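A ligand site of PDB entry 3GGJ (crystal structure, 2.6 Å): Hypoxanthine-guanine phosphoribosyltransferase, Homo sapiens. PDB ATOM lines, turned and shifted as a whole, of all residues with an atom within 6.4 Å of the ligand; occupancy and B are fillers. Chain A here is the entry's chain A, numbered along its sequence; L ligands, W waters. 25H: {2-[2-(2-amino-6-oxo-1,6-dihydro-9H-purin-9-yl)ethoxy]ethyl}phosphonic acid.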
ATOM      1  N   LYS A  68     -25.341  -1.515   3.198  1.00  0.00           N
ATOM      2  CA  LYS A  68     -25.997  -0.259   2.872  1.00  0.00           C
ATOM      3  C   LYS A  68     -26.198  -0.152   1.371  1.00  0.00           C
ATOM      4  O   LYS A  68     -27.276  -0.443   0.879  1.00  0.00           O
ATOM      5  CB  LYS A  68     -25.225   0.956   3.401  1.00  0.00           C
ATOM      6  CG  LYS A  68     -25.611   1.375   4.812  1.00  0.00           C
ATOM      7  CD  LYS A  68     -24.572   0.973   5.824  1.00  0.00           C
ATOM      8  CE  LYS A  68     -23.395   1.966   5.853  1.00  0.00           C
ATOM      9  NZ  LYS A  68     -22.305   1.644   4.870  1.00  0.00           N
ATOM     10  N   ASP A 107     -28.092  11.608   8.025  1.00  0.00           N
ATOM     11  CA  ASP A 107     -26.960  11.071   8.781  1.00  0.00           C
ATOM     12  C   ASP A 107     -26.638  11.915  10.022  1.00  0.00           C
ATOM     13  O   ASP A 107     -25.486  11.952  10.469  1.00  0.00           O
ATOM     14  CB  ASP A 107     -25.732  10.949   7.878  1.00  0.00           C
ATOM     15  CG  ASP A 107     -24.860   9.754   8.231  1.00  0.00           C
ATOM     16  OD1 ASP A 107     -25.075   9.153   9.307  1.00  0.00           O
ATOM     17  OD2 ASP A 107     -23.951   9.420   7.429  1.00  0.00           O
ATOM     18  N   THR A 110     -27.184   8.444  13.055  1.00  0.00           N
ATOM     19  CA  THR A 110     -26.949   7.178  12.367  1.00  0.00           C
ATOM     20  C   THR A 110     -27.158   5.978  13.294  1.00  0.00           C
ATOM     21  O   THR A 110     -27.256   4.828  12.827  1.00  0.00           O
ATOM     22  CB  THR A 110     -25.533   7.101  11.764  1.00  0.00           C
ATOM     23  OG1 THR A 110     -24.913   8.394  11.819  1.00  0.00           O
ATOM     24  CG2 THR A 110     -25.598   6.620  10.318  1.00  0.00           C
ATOM     25  N   GLY A 111     -27.213   6.255  14.604  1.00  0.00           N
ATOM     26  CA  GLY A 111     -27.390   5.224  15.625  1.00  0.00           C
ATOM     27  C   GLY A 111     -28.740   4.541  15.519  1.00  0.00           C
ATOM     28  O   GLY A 111     -28.926   3.423  15.992  1.00  0.00           O
ATOM     29  N   GLU A 133     -18.199  -4.494   7.838  1.00  0.00           N
ATOM     30  CA  GLU A 133     -18.587  -3.123   7.528  1.00  0.00           C
ATOM     31  C   GLU A 133     -17.508  -2.466   6.658  1.00  0.00           C
ATOM     32  O   GLU A 133     -16.342  -2.875   6.694  1.00  0.00           O
ATOM     33  CB  GLU A 133     -18.770  -2.340   8.831  1.00  0.00           C
ATOM     34  CG  GLU A 133     -19.211  -0.900   8.682  1.00  0.00           C
ATOM     35  CD  GLU A 133     -20.649  -0.761   8.219  1.00  0.00           C
ATOM     36  OE1 GLU A 133     -21.456  -0.212   9.000  1.00  0.00           O
ATOM     37  OE2 GLU A 133     -20.966  -1.187   7.077  1.00  0.00           O
ATOM     38  N   ASP A 134     -17.883  -1.454   5.877  1.00  0.00           N
ATOM     39  CA  ASP A 134     -16.946  -0.810   4.966  1.00  0.00           C
ATOM     40  C   ASP A 134     -16.312   0.448   5.550  1.00  0.00           C
ATOM     41  O   ASP A 134     -15.103   0.670   5.412  1.00  0.00           O
ATOM     42  CB  ASP A 134     -17.619  -0.511   3.615  1.00  0.00           C
ATOM     43  CG  ASP A 134     -18.927   0.249   3.775  1.00  0.00           C
ATOM     44  OD1 ASP A 134     -19.154   0.861   4.842  1.00  0.00           O
ATOM     45  OD2 ASP A 134     -19.742   0.225   2.822  1.00  0.00           O
ATOM     46  N   ILE A 135     -17.112   1.278   6.194  1.00  0.00           N
ATOM     47  CA  ILE A 135     -16.603   2.461   6.873  1.00  0.00           C
ATOM     48  C   ILE A 135     -17.279   2.622   8.241  1.00  0.00           C
ATOM     49  O   ILE A 135     -18.452   2.273   8.400  1.00  0.00           O
ATOM     50  CB  ILE A 135     -16.800   3.717   5.993  1.00  0.00           C
ATOM     51  CG1 ILE A 135     -16.206   4.968   6.659  1.00  0.00           C
ATOM     52  CG2 ILE A 135     -18.271   3.883   5.598  1.00  0.00           C
ATOM     53  CD1 ILE A 135     -15.765   6.016   5.677  1.00  0.00           C
ATOM     54  N   ILE A 136     -16.520   3.097   9.233  1.00  0.00           N
ATOM     55  CA  ILE A 136     -17.087   3.505  10.520  1.00  0.00           C
ATOM     56  C   ILE A 136     -16.680   4.955  10.714  1.00  0.00           C
ATOM     57  O   ILE A 136     -15.515   5.319  10.557  1.00  0.00           O
ATOM     58  CB  ILE A 136     -16.543   2.645  11.713  1.00  0.00           C
ATOM     59  CG1 ILE A 136     -17.097   1.217  11.674  1.00  0.00           C
ATOM     60  CG2 ILE A 136     -16.877   3.302  13.087  1.00  0.00           C
ATOM     61  CD1 ILE A 136     -16.350   0.263  12.604  1.00  0.00           C
ATOM     62  N   ASP A 137     -17.664   5.777  11.062  1.00  0.00           N
ATOM     63  CA  ASP A 137     -17.441   7.200  11.220  1.00  0.00           C
ATOM     64  C   ASP A 137     -17.668   7.570  12.693  1.00  0.00           C
ATOM     65  O   ASP A 137     -16.749   7.454  13.510  1.00  0.00           O
ATOM     66  CB  ASP A 137     -18.362   7.964  10.249  1.00  0.00           C
ATOM     67  CG  ASP A 137     -18.155   9.472  10.292  1.00  0.00           C
ATOM     68  OD1 ASP A 137     -17.008   9.914  10.538  1.00  0.00           O
ATOM     69  OD2 ASP A 137     -19.150  10.213  10.086  1.00  0.00           O
ATOM     70  N   THR A 138     -18.883   7.986  13.047  1.00  0.00           N
ATOM     71  CA  THR A 138     -19.198   8.317  14.431  1.00  0.00           C
ATOM     72  C   THR A 138     -19.243   7.059  15.292  1.00  0.00           C
ATOM     73  O   THR A 138     -19.091   7.133  16.524  1.00  0.00           O
ATOM     74  CB  THR A 138     -20.552   9.048  14.568  1.00  0.00           C
ATOM     75  OG1 THR A 138     -21.618   8.170  14.198  1.00  0.00           O
ATOM     76  CG2 THR A 138     -20.587  10.301  13.705  1.00  0.00           C
ATOM     77  N   GLY A 139     -19.461   5.915  14.661  1.00  0.00           N
ATOM     78  CA  GLY A 139     -19.518   4.631  15.357  1.00  0.00           C
ATOM     79  C   GLY A 139     -20.894   4.240  15.866  1.00  0.00           C
ATOM     80  O   GLY A 139     -21.055   3.139  16.389  1.00  0.00           O
ATOM     81  N   LYS A 140     -21.876   5.125  15.693  1.00  0.00           N
ATOM     82  CA  LYS A 140     -23.248   4.912  16.213  1.00  0.00           C
ATOM     83  C   LYS A 140     -24.063   3.799  15.511  1.00  0.00           C
ATOM     84  O   LYS A 140     -24.862   3.119  16.155  1.00  0.00           O
ATOM     85  CB  LYS A 140     -24.054   6.220  16.175  1.00  0.00           C
ATOM     86  CG  LYS A 140     -23.551   7.293  17.113  1.00  0.00           C
ATOM     87  CD  LYS A 140     -24.459   8.516  17.034  1.00  0.00           C
ATOM     88  CE  LYS A 140     -23.791   9.770  17.570  1.00  0.00           C
ATOM     89  NZ  LYS A 140     -24.366  10.996  16.950  1.00  0.00           N
ATOM     90  N   THR A 141     -23.876   3.619  14.211  1.00  0.00           N
ATOM     91  CA  THR A 141     -24.557   2.545  13.505  1.00  0.00           C
ATOM     92  C   THR A 141     -24.187   1.218  14.127  1.00  0.00           C
ATOM     93  O   THR A 141     -25.039   0.430  14.528  1.00  0.00           O
ATOM     94  CB  THR A 141     -24.158   2.525  12.026  1.00  0.00           C
ATOM     95  OG1 THR A 141     -24.601   3.734  11.406  1.00  0.00           O
ATOM     96  CG2 THR A 141     -24.764   1.335  11.307  1.00  0.00           C
ATOM     97  N   MET A 142     -22.881   0.993  14.227  1.00  0.00           N
ATOM     98  CA  MET A 142     -22.349  -0.287  14.667  1.00  0.00           C
ATOM     99  C   MET A 142     -22.714  -0.605  16.096  1.00  0.00           C
ATOM    100  O   MET A 142     -23.161  -1.708  16.386  1.00  0.00           O
ATOM    101  CB  MET A 142     -20.832  -0.310  14.484  1.00  0.00           C
ATOM    102  CG  MET A 142     -20.283  -1.708  14.554  1.00  0.00           C
ATOM    103  SD  MET A 142     -20.999  -2.776  13.302  1.00  0.00           S
ATOM    104  CE  MET A 142     -20.323  -2.096  11.807  1.00  0.00           C
ATOM    105  N   LYS A 165     -12.721   6.083  10.523  1.00  0.00           N
ATOM    106  CA  LYS A 165     -12.438   7.507  10.410  1.00  0.00           C
ATOM    107  C   LYS A 165     -12.037   8.052  11.763  1.00  0.00           C
ATOM    108  O   LYS A 165     -12.687   7.776  12.768  1.00  0.00           O
ATOM    109  CB  LYS A 165     -13.665   8.249   9.922  1.00  0.00           C
ATOM    110  CG  LYS A 165     -13.404   9.459   9.056  1.00  0.00           C
ATOM    111  CD  LYS A 165     -14.402   9.460   7.898  1.00  0.00           C
ATOM    112  CE  LYS A 165     -14.816  10.863   7.528  1.00  0.00           C
ATOM    113  NZ  LYS A 165     -16.004  10.824   6.628  1.00  0.00           N
ATOM    114  N   ARG A 169     -16.079  13.322  16.382  1.00  0.00           N
ATOM    115  CA  ARG A 169     -17.489  12.933  16.397  1.00  0.00           C
ATOM    116  C   ARG A 169     -17.659  11.441  16.689  1.00  0.00           C
ATOM    117  O   ARG A 169     -18.775  10.953  16.822  1.00  0.00           O
ATOM    118  CB  ARG A 169     -18.184  13.321  15.082  1.00  0.00           C
ATOM    119  CG  ARG A 169     -18.451  14.811  14.896  1.00  0.00           C
ATOM    120  CD  ARG A 169     -18.645  15.189  13.424  1.00  0.00           C
ATOM    121  NE  ARG A 169     -19.224  14.074  12.680  1.00  0.00           N
ATOM    122  CZ  ARG A 169     -18.554  13.344  11.794  1.00  0.00           C
ATOM    123  NH1 ARG A 169     -17.293  13.611  11.503  1.00  0.00           N
ATOM    124  NH2 ARG A 169     -19.164  12.339  11.185  1.00  0.00           N
ATOM    125  N   ILE A 182      -8.217   6.459   8.880  1.00  0.00           N
ATOM    126  CA  ILE A 182      -8.113   7.552   7.907  1.00  0.00           C
ATOM    127  C   ILE A 182      -8.492   8.913   8.486  1.00  0.00           C
ATOM    128  O   ILE A 182      -9.164   8.973   9.521  1.00  0.00           O
ATOM    129  CB  ILE A 182      -8.973   7.237   6.632  1.00  0.00           C
ATOM    130  CG1 ILE A 182     -10.464   7.081   7.010  1.00  0.00           C
ATOM    131  CG2 ILE A 182      -8.444   5.965   5.961  1.00  0.00           C
ATOM    132  CD1 ILE A 182     -11.448   7.520   5.922  1.00  0.00           C
ATOM    133  N   LYS A 185     -12.138  13.207   6.605  1.00  0.00           N
ATOM    134  CA  LYS A 185     -12.564  13.737   5.303  1.00  0.00           C
ATOM    135  C   LYS A 185     -13.517  12.758   4.643  1.00  0.00           C
ATOM    136  O   LYS A 185     -13.457  11.562   4.895  1.00  0.00           O
ATOM    137  CB  LYS A 185     -11.358  13.929   4.409  1.00  0.00           C
ATOM    138  CG  LYS A 185     -10.502  15.123   4.766  1.00  0.00           C
ATOM    139  CD  LYS A 185      -9.135  15.009   4.133  1.00  0.00           C
ATOM    140  CE  LYS A 185      -8.269  16.237   4.460  1.00  0.00           C
ATOM    141  NZ  LYS A 185      -6.820  16.022   4.132  1.00  0.00           N
ATOM    142  N   PHE A 186     -14.412  13.260   3.784  1.00  0.00           N
ATOM    143  CA  PHE A 186     -15.433  12.421   3.172  1.00  0.00           C
ATOM    144  C   PHE A 186     -14.939  11.670   1.916  1.00  0.00           C
ATOM    145  O   PHE A 186     -14.693  12.280   0.880  1.00  0.00           O
ATOM    146  CB  PHE A 186     -16.670  13.245   2.841  1.00  0.00           C
ATOM    147  CG  PHE A 186     -17.866  12.432   2.443  1.00  0.00           C
ATOM    148  CD1 PHE A 186     -18.852  12.117   3.374  1.00  0.00           C
ATOM    149  CD2 PHE A 186     -18.007  11.963   1.142  1.00  0.00           C
ATOM    150  CE1 PHE A 186     -19.954  11.361   3.006  1.00  0.00           C
ATOM    151  CE2 PHE A 186     -19.099  11.206   0.770  1.00  0.00           C
ATOM    152  CZ  PHE A 186     -20.076  10.904   1.696  1.00  0.00           C
ATOM    153  N   VAL A 187     -14.854  10.349   2.022  1.00  0.00           N
ATOM    154  CA  VAL A 187     -14.276   9.537   0.949  1.00  0.00           C
ATOM    155  C   VAL A 187     -15.297   8.733   0.123  1.00  0.00           C
ATOM    156  O   VAL A 187     -16.395   8.409   0.582  1.00  0.00           O
ATOM    157  CB  VAL A 187     -13.149   8.587   1.465  1.00  0.00           C
ATOM    158  CG1 VAL A 187     -11.977   9.399   2.047  1.00  0.00           C
ATOM    159  CG2 VAL A 187     -13.688   7.564   2.468  1.00  0.00           C
ATOM    160  N   VAL A 188     -14.897   8.432  -1.107  1.00  0.00           N
ATOM    161  CA  VAL A 188     -15.676   7.629  -2.031  1.00  0.00           C
ATOM    162  C   VAL A 188     -14.732   6.662  -2.752  1.00  0.00           C
ATOM    163  O   VAL A 188     -13.509   6.813  -2.689  1.00  0.00           O
ATOM    164  CB  VAL A 188     -16.386   8.503  -3.085  1.00  0.00           C
ATOM    165  CG1 VAL A 188     -17.453   9.384  -2.427  1.00  0.00           C
ATOM    166  CG2 VAL A 188     -15.375   9.340  -3.838  1.00  0.00           C
ATOM    167  N   LEU A 192     -17.452   2.512  -1.416  1.00  0.00           N
ATOM    168  CA  LEU A 192     -18.296   3.635  -1.065  1.00  0.00           C
ATOM    169  C   LEU A 192     -18.775   4.443  -2.279  1.00  0.00           C
ATOM    170  O   LEU A 192     -17.980   5.084  -2.973  1.00  0.00           O
ATOM    171  CB  LEU A 192     -17.577   4.524  -0.046  1.00  0.00           C
ATOM    172  CG  LEU A 192     -17.097   3.768   1.188  1.00  0.00           C
ATOM    173  CD1 LEU A 192     -16.356   4.699   2.108  1.00  0.00           C
ATOM    174  CD2 LEU A 192     -18.271   3.153   1.920  1.00  0.00           C
ATOM    175  N   ASP A 193     -20.085   4.380  -2.540  1.00  0.00           N
ATOM    176  CA  ASP A 193     -20.719   5.151  -3.608  1.00  0.00           C
ATOM    177  C   ASP A 193     -21.165   6.511  -3.075  1.00  0.00           C
ATOM    178  O   ASP A 193     -21.218   6.737  -1.873  1.00  0.00           O
ATOM    179  CB  ASP A 193     -21.896   4.386  -4.229  1.00  0.00           C
ATOM    180  CG  ASP A 193     -23.196   4.525  -3.411  1.00  0.00           C
ATOM    181  OD1 ASP A 193     -23.426   3.686  -2.502  1.00  0.00           O
ATOM    182  OD2 ASP A 193     -23.978   5.455  -3.682  1.00  0.00           O
ATOM    183  N   TYR A 194     -21.485   7.427  -3.987  1.00  0.00           N
ATOM    184  CA  TYR A 194     -22.048   8.715  -3.622  1.00  0.00           C
ATOM    185  C   TYR A 194     -23.257   8.931  -4.527  1.00  0.00           C
ATOM    186  O   TYR A 194     -23.108   9.170  -5.724  1.00  0.00           O
ATOM    187  CB  TYR A 194     -21.018   9.826  -3.781  1.00  0.00           C
ATOM    188  CG  TYR A 194     -21.515  11.201  -3.359  1.00  0.00           C
ATOM    189  CD1 TYR A 194     -21.583  11.551  -2.015  1.00  0.00           C
ATOM    190  CD2 TYR A 194     -21.904  12.145  -4.302  1.00  0.00           C
ATOM    191  CE1 TYR A 194     -22.034  12.795  -1.622  1.00  0.00           C
ATOM    192  CE2 TYR A 194     -22.358  13.410  -3.917  1.00  0.00           C
ATOM    193  CZ  TYR A 194     -22.417  13.717  -2.574  1.00  0.00           C
ATOM    194  OH  TYR A 194     -22.860  14.960  -2.185  1.00  0.00           O
HETATM  195  N1  25H L   1     -17.795   8.437   3.037  1.00  0.00           N
HETATM  196  C8  25H L   1     -19.931   8.694   7.009  1.00  0.00           C
HETATM  197  C6  25H L   1     -17.609   8.923   4.292  1.00  0.00           C
HETATM  198  N7  25H L   1     -18.716   9.128   6.551  1.00  0.00           N
HETATM  199  C5  25H L   1     -18.619   8.760   5.249  1.00  0.00           C
HETATM  200  C2  25H L   1     -18.954   7.799   2.721  1.00  0.00           C
HETATM  201  OAD 25H L   1     -21.158   7.179  11.413  1.00  0.00           O
HETATM  202  PAT 25H L   1     -21.331   5.683  11.557  1.00  0.00           P
HETATM  203  OAE 25H L   1     -22.654   5.285  12.182  1.00  0.00           O
HETATM  204  OAC 25H L   1     -20.121   5.000  12.167  1.00  0.00           O
HETATM  205  CAJ 25H L   1     -21.446   4.997   9.888  1.00  0.00           C
HETATM  206  CAH 25H L   1     -21.667   6.132   8.902  1.00  0.00           C
HETATM  207  OAN 25H L   1     -20.966   5.812   7.703  1.00  0.00           O
HETATM  208  CAG 25H L   1     -21.789   6.000   6.539  1.00  0.00           C
HETATM  209  CAI 25H L   1     -21.903   7.477   6.116  1.00  0.00           C
HETATM  210  N9  25H L   1     -20.579   8.082   6.011  1.00  0.00           N
HETATM  211  C4  25H L   1     -19.793   8.099   4.902  1.00  0.00           C
HETATM  212  N3  25H L   1     -19.940   7.618   3.636  1.00  0.00           N
HETATM  213  N2  25H L   1     -19.134   7.314   1.479  1.00  0.00           N
HETATM  214  O6  25H L   1     -16.508   9.557   4.628  1.00  0.00           O
HETATM  215  O   HOH W   1     -21.116   5.099   0.099  1.00  0.00           O
HETATM  216  O   HOH W   2     -21.089   2.658  13.009  1.00  0.00           O
HETATM  217  O   HOH W   3     -19.396  12.021   8.046  1.00  0.00           O
HETATM  218  O   HOH W   4     -21.391   2.453   7.681  1.00  0.00           O
HETATM  219  O   HOH W   5     -21.465   9.546  10.467  1.00  0.00           O
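NZ of Lys 165 sits at hydrogen-bond distance from O6 of the ligand, 2.4 Å away.
The backbone NH (N) of Thr 141 sits at hydrogen-bond distance from an oxygen (OAE) of the ligand, 2.9 Å away.
OG1 of Thr 141 is in hydrogen-bond range of OAE of the ligand (2.6 Å).
An oxygen (OAC) of the ligand sits at hydrogen-bond distance from the backbone NH (N) of Gly 139, at 2.7 Å.
N of Asp 137 lies within hydrogen-bond range of OAC of the ligand (2.8 Å).
N of Val 187 is in hydrogen-bond range of O6 of the ligand, at 3.2 Å.
N1 of the ligand sits at hydrogen-bond distance from O of Val 187.
The backbone NH of Thr 138 is in hydrogen-bond range of an oxygen (OAD) of the ligand (2.9 Å).
OG1 of Thr 138 sits at hydrogen-bond distance from OAD of the ligand, 3.0 Å away.
The side-chain amino group (NZ) of Lys 165 sits close to the backbone carbonyl oxygen (O) of Lys 185.
The backbone NH (N) of Lys 165 sits at hydrogen-bond distance from the backbone carbonyl oxygen (O) of Ile 136 (2.9 Å).
OG1 of Thr 141 is in hydrogen-bond range of O of Thr 110.
OD1 of Asp 137 lies within salt-bridge range of NH2 of Arg 169.
N of Lys 140 lies close to OG1 of Thr 138 (3.4 Å).
OG1 of Thr 110 lies within hydrogen-bond range of OD1 of Asp 107, 2.6 Å away.
Residues that only touch the ligand: Asp 107, Phe 186, Thr 110, Leu 192, Lys 140, Lys 185, Ile 135, Ile 136 and Asp 193.
15 residues have an atom within 4 Å of the ligand: Asp 107, Thr 110, Ile 135, Ile 136, Asp 137, Thr 138, Gly 139, Lys 140, Thr 141, Lys 165, Lys 185, Phe 186, Val 187, Leu 192 and Asp 193.
The nearest printed residue that does not touch the ligand is Lys 68 (4.4 Å).
Water W5 lies within hydrogen-bond range of OD2 of Asp 137 (2.4 Å) and OAD of the ligand (2.6 Å).
Water W2 lies within hydrogen-bond range of OAC of the ligand (2.7 Å), N of Met 142 (2.7 Å), N of Thr 141 (3.2 Å) and O of Gly 139 (3.4 Å).
Water W1 bridges O of Asp 193 (2.6 Å) and N2 of the ligand (3.3 Å).
Water W3 lies within hydrogen-bond range of OD2 of Asp 137 (2.7 Å), NH2 of Arg 169 (3.2 Å) and N7 of the ligand (3.3 Å).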
